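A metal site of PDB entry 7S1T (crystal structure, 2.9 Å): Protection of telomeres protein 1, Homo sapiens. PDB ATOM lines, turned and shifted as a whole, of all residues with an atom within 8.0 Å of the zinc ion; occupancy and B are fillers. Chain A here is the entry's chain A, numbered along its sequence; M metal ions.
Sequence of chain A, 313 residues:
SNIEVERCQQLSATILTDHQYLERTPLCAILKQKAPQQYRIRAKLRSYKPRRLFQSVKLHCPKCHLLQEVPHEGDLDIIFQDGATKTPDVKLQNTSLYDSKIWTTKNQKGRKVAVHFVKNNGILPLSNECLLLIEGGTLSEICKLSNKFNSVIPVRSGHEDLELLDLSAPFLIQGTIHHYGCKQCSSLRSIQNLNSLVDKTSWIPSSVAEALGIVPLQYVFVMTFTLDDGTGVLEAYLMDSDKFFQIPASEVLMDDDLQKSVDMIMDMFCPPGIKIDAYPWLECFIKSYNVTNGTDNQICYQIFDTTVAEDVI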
ATOM      1  N   HIS A  60      -4.410  20.284  22.705  1.00  0.00           N
ATOM      2  CA  HIS A  60      -5.382  19.217  22.557  1.00  0.00           C
ATOM      3  C   HIS A  60      -6.013  18.886  23.903  1.00  0.00           C
ATOM      4  O   HIS A  60      -5.303  18.692  24.893  1.00  0.00           O
ATOM      5  CB  HIS A  60      -4.730  17.964  21.965  1.00  0.00           C
ATOM      6  CG  HIS A  60      -5.698  16.890  21.603  1.00  0.00           C
ATOM      7  ND1 HIS A  60      -6.350  16.851  20.386  1.00  0.00           N
ATOM      8  CD2 HIS A  60      -6.130  15.801  22.282  1.00  0.00           C
ATOM      9  CE1 HIS A  60      -7.142  15.793  20.339  1.00  0.00           C
ATOM     10  NE2 HIS A  60      -7.027  15.137  21.483  1.00  0.00           N
ATOM     11  N   CYS A  61      -7.338  18.841  23.944  1.00  0.00           N
ATOM     12  CA  CYS A  61      -8.029  18.380  25.132  1.00  0.00           C
ATOM     13  C   CYS A  61      -8.109  16.864  25.081  1.00  0.00           C
ATOM     14  O   CYS A  61      -8.786  16.303  24.209  1.00  0.00           O
ATOM     15  CB  CYS A  61      -9.437  18.985  25.233  1.00  0.00           C
ATOM     16  SG  CYS A  61     -10.446  18.258  26.536  1.00  0.00           S
ATOM     17  N   PRO A  62      -7.433  16.159  25.992  1.00  0.00           N
ATOM     18  CA  PRO A  62      -7.371  14.687  25.894  1.00  0.00           C
ATOM     19  C   PRO A  62      -8.732  14.012  25.877  1.00  0.00           C
ATOM     20  O   PRO A  62      -8.889  12.993  25.203  1.00  0.00           O
ATOM     21  CB  PRO A  62      -6.546  14.295  27.131  1.00  0.00           C
ATOM     22  CG  PRO A  62      -5.714  15.503  27.426  1.00  0.00           C
ATOM     23  CD  PRO A  62      -6.590  16.674  27.089  1.00  0.00           C
ATOM     24  N   LYS A  63      -9.714  14.542  26.605  1.00  0.00           N
ATOM     25  CA  LYS A  63     -11.034  13.906  26.615  1.00  0.00           C
ATOM     26  C   LYS A  63     -11.834  14.271  25.362  1.00  0.00           C
ATOM     27  O   LYS A  63     -11.995  13.434  24.469  1.00  0.00           O
ATOM     28  CB  LYS A  63     -11.802  14.297  27.883  1.00  0.00           C
ATOM     29  CG  LYS A  63     -13.063  13.473  28.135  1.00  0.00           C
ATOM     30  CD  LYS A  63     -12.972  12.065  27.533  1.00  0.00           C
ATOM     31  CE  LYS A  63     -13.855  11.066  28.270  1.00  0.00           C
ATOM     32  NZ  LYS A  63     -15.306  11.300  28.035  1.00  0.00           N
ATOM     33  N   CYS A  64     -12.335  15.497  25.290  1.00  0.00           N
ATOM     34  CA  CYS A  64     -13.214  15.905  24.196  1.00  0.00           C
ATOM     35  C   CYS A  64     -12.468  16.131  22.885  1.00  0.00           C
ATOM     36  O   CYS A  64     -13.085  16.618  21.929  1.00  0.00           O
ATOM     37  CB  CYS A  64     -14.013  17.153  24.579  1.00  0.00           C
ATOM     38  SG  CYS A  64     -13.135  18.716  24.440  1.00  0.00           S
ATOM     39  N   HIS A  65     -11.181  15.791  22.824  1.00  0.00           N
ATOM     40  CA  HIS A  65     -10.383  15.862  21.583  1.00  0.00           C
ATOM     41  C   HIS A  65     -10.487  17.235  20.927  1.00  0.00           C
ATOM     42  O   HIS A  65     -10.429  17.368  19.704  1.00  0.00           O
ATOM     43  CB  HIS A  65     -10.797  14.751  20.618  1.00  0.00           C
ATOM     44  CG  HIS A  65     -10.376  13.386  21.056  1.00  0.00           C
ATOM     45  ND1 HIS A  65     -11.026  12.687  22.048  1.00  0.00           N
ATOM     46  CD2 HIS A  65      -9.342  12.592  20.662  1.00  0.00           C
ATOM     47  CE1 HIS A  65     -10.430  11.529  22.237  1.00  0.00           C
ATOM     48  NE2 HIS A  65      -9.409  11.441  21.404  1.00  0.00           N
ATOM     49  N   LEU A  66     -10.609  18.261  21.750  1.00  0.00           N
ATOM     50  CA  LEU A  66     -10.648  19.640  21.270  1.00  0.00           C
ATOM     51  C   LEU A  66      -9.259  20.081  20.831  1.00  0.00           C
ATOM     52  O   LEU A  66      -8.296  19.972  21.599  1.00  0.00           O
ATOM     53  CB  LEU A  66     -11.163  20.558  22.382  1.00  0.00           C
ATOM     54  CG  LEU A  66     -11.539  22.020  22.111  1.00  0.00           C
ATOM     55  CD1 LEU A  66     -12.603  22.123  21.029  1.00  0.00           C
ATOM     56  CD2 LEU A  66     -12.002  22.674  23.402  1.00  0.00           C
ATOM     57  N   GLN A  68      -7.305  23.437  19.805  1.00  0.00           N
ATOM     58  CA  GLN A  68      -7.441  24.883  19.878  1.00  0.00           C
ATOM     59  C   GLN A  68      -6.058  25.514  19.956  1.00  0.00           C
ATOM     60  O   GLN A  68      -5.048  24.823  20.097  1.00  0.00           O
ATOM     61  CB  GLN A  68      -8.307  25.297  21.076  1.00  0.00           C
ATOM     62  CG  GLN A  68      -7.609  25.172  22.419  1.00  0.00           C
ATOM     63  CD  GLN A  68      -8.378  25.846  23.536  1.00  0.00           C
ATOM     64  OE1 GLN A  68      -9.363  25.318  24.040  1.00  0.00           O
ATOM     65  NE2 GLN A  68      -7.918  27.035  23.923  1.00  0.00           N
ATOM     66  N   GLY A 181      -6.859  24.667  31.273  1.00  0.00           N
ATOM     67  CA  GLY A 181      -7.923  23.692  31.360  1.00  0.00           C
ATOM     68  C   GLY A 181      -8.924  23.883  30.232  1.00  0.00           C
ATOM     69  O   GLY A 181      -9.143  24.991  29.766  1.00  0.00           O
ATOM     70  N   CYS A 182      -9.515  22.779  29.791  1.00  0.00           N
ATOM     71  CA  CYS A 182     -10.525  22.842  28.741  1.00  0.00           C
ATOM     72  C   CYS A 182     -11.783  23.530  29.257  1.00  0.00           C
ATOM     73  O   CYS A 182     -12.339  23.129  30.277  1.00  0.00           O
ATOM     74  CB  CYS A 182     -10.861  21.435  28.235  1.00  0.00           C
ATOM     75  SG  CYS A 182     -11.999  21.401  26.828  1.00  0.00           S
ATOM     76  N   LYS A 183     -12.218  24.560  28.547  1.00  0.00           N
ATOM     77  CA  LYS A 183     -13.369  25.329  28.996  1.00  0.00           C
ATOM     78  C   LYS A 183     -14.682  24.568  28.844  1.00  0.00           C
ATOM     79  O   LYS A 183     -15.677  24.968  29.464  1.00  0.00           O
ATOM     80  CB  LYS A 183     -13.464  26.646  28.219  1.00  0.00           C
ATOM     81  CG  LYS A 183     -12.545  27.722  28.728  1.00  0.00           C
ATOM     82  CD  LYS A 183     -12.888  29.070  28.113  1.00  0.00           C
ATOM     83  CE  LYS A 183     -11.977  30.158  28.642  1.00  0.00           C
ATOM     84  NZ  LYS A 183     -12.009  31.377  27.775  1.00  0.00           N
ATOM     85  N   GLN A 184     -14.702  23.498  28.070  1.00  0.00           N
ATOM     86  CA  GLN A 184     -15.948  22.796  27.771  1.00  0.00           C
ATOM     87  C   GLN A 184     -16.176  21.554  28.610  1.00  0.00           C
ATOM     88  O   GLN A 184     -17.328  21.114  28.740  1.00  0.00           O
ATOM     89  CB  GLN A 184     -16.002  22.416  26.291  1.00  0.00           C
ATOM     90  CG  GLN A 184     -16.404  23.557  25.365  1.00  0.00           C
ATOM     91  CD  GLN A 184     -17.488  23.163  24.386  1.00  0.00           C
ATOM     92  OE1 GLN A 184     -18.529  22.630  24.781  1.00  0.00           O
ATOM     93  NE2 GLN A 184     -17.251  23.421  23.111  1.00  0.00           N
ATOM     94  N   CYS A 185     -15.131  20.969  29.197  1.00  0.00           N
ATOM     95  CA  CYS A 185     -15.279  19.726  29.937  1.00  0.00           C
ATOM     96  C   CYS A 185     -14.580  19.816  31.297  1.00  0.00           C
ATOM     97  O   CYS A 185     -13.990  18.849  31.769  1.00  0.00           O
ATOM     98  CB  CYS A 185     -14.747  18.539  29.135  1.00  0.00           C
ATOM     99  SG  CYS A 185     -12.956  18.513  28.899  1.00  0.00           S
ATOM    100  N   SER A 186     -14.672  20.968  31.954  1.00  0.00           N
ATOM    101  CA  SER A 186     -14.057  21.134  33.277  1.00  0.00           C
ATOM    102  C   SER A 186     -14.872  22.173  34.049  1.00  0.00           C
ATOM    103  O   SER A 186     -14.695  23.374  33.844  1.00  0.00           O
ATOM    104  CB  SER A 186     -12.602  21.545  33.156  1.00  0.00           C
ATOM    105  OG  SER A 186     -12.476  22.902  32.803  1.00  0.00           O
ATOM    106  N   VAL A 215      -9.820  19.969  33.866  1.00  0.00           N
ATOM    107  CA  VAL A 215      -9.295  18.963  32.947  1.00  0.00           C
ATOM    108  C   VAL A 215      -8.293  19.655  32.031  1.00  0.00           C
ATOM    109  O   VAL A 215      -8.704  20.452  31.165  1.00  0.00           O
ATOM    110  CB  VAL A 215     -10.418  18.290  32.153  1.00  0.00           C
ATOM    111  CG1 VAL A 215      -9.871  17.164  31.299  1.00  0.00           C
ATOM    112  CG2 VAL A 215     -11.462  17.755  33.119  1.00  0.00           C
ATOM    113  N   PRO A 216      -6.995  19.402  32.175  1.00  0.00           N
ATOM    114  CA  PRO A 216      -5.993  20.206  31.480  1.00  0.00           C
ATOM    115  C   PRO A 216      -5.873  19.872  30.000  1.00  0.00           C
ATOM    116  O   PRO A 216      -6.095  18.739  29.572  1.00  0.00           O
ATOM    117  CB  PRO A 216      -4.694  19.865  32.218  1.00  0.00           C
ATOM    118  CG  PRO A 216      -4.918  18.482  32.737  1.00  0.00           C
ATOM    119  CD  PRO A 216      -6.393  18.388  33.056  1.00  0.00           C
ATOM    120  N   LEU A 217      -5.519  20.882  29.226  1.00  0.00           N
ATOM    121  CA  LEU A 217      -5.217  20.711  27.816  1.00  0.00           C
ATOM    122  C   LEU A 217      -3.776  20.211  27.639  1.00  0.00           C
ATOM    123  O   LEU A 217      -2.939  20.319  28.550  1.00  0.00           O
ATOM    124  CB  LEU A 217      -5.401  22.024  27.054  1.00  0.00           C
ATOM    125  CG  LEU A 217      -6.766  22.705  27.147  1.00  0.00           C
ATOM    126  CD1 LEU A 217      -6.704  24.110  26.556  1.00  0.00           C
ATOM    127  CD2 LEU A 217      -7.807  21.883  26.435  1.00  0.00           C
HETATM  128 ZN    ZN M   1     -12.674  19.102  26.686  1.00  0.00          ZN
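The backbone carbonyl oxygen of Cys 182 lies within hydrogen-bond range of the side-chain hydroxyl of Ser 186 (2.5 Å). The backbone carbonyl oxygen (O) of Leu 66 lies within hydrogen-bond range of the backbone NH (N) of Cys 61, at 2.8 Å. The backbone NH of Cys 182 is in hydrogen-bond range of the backbone carbonyl oxygen of Val 215 (2.8 Å). The side-chain sulfur (SG) of Cys 61 lies close to the backbone NH (N) of Lys 63 (3.8 Å). N of Leu 66 sits close to SG of Cys 64, at 3.7 Å. The side-chain sulfur of Cys 182 lies close to the backbone NH of Gln 184 (3.6 Å).
Within 4 Å of the zinc ion: Cys 61, Cys 64, Cys 182 and Cys 185.
The zinc ion is bound by the side-chain sulfur of Cys 185 (2.3 Å), the side-chain sulfur of Cys 64 (2.3 Å), the side-chain sulfur of Cys 61 (2.4 Å) and the side-chain sulfur of Cys 182 (2.4 Å).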
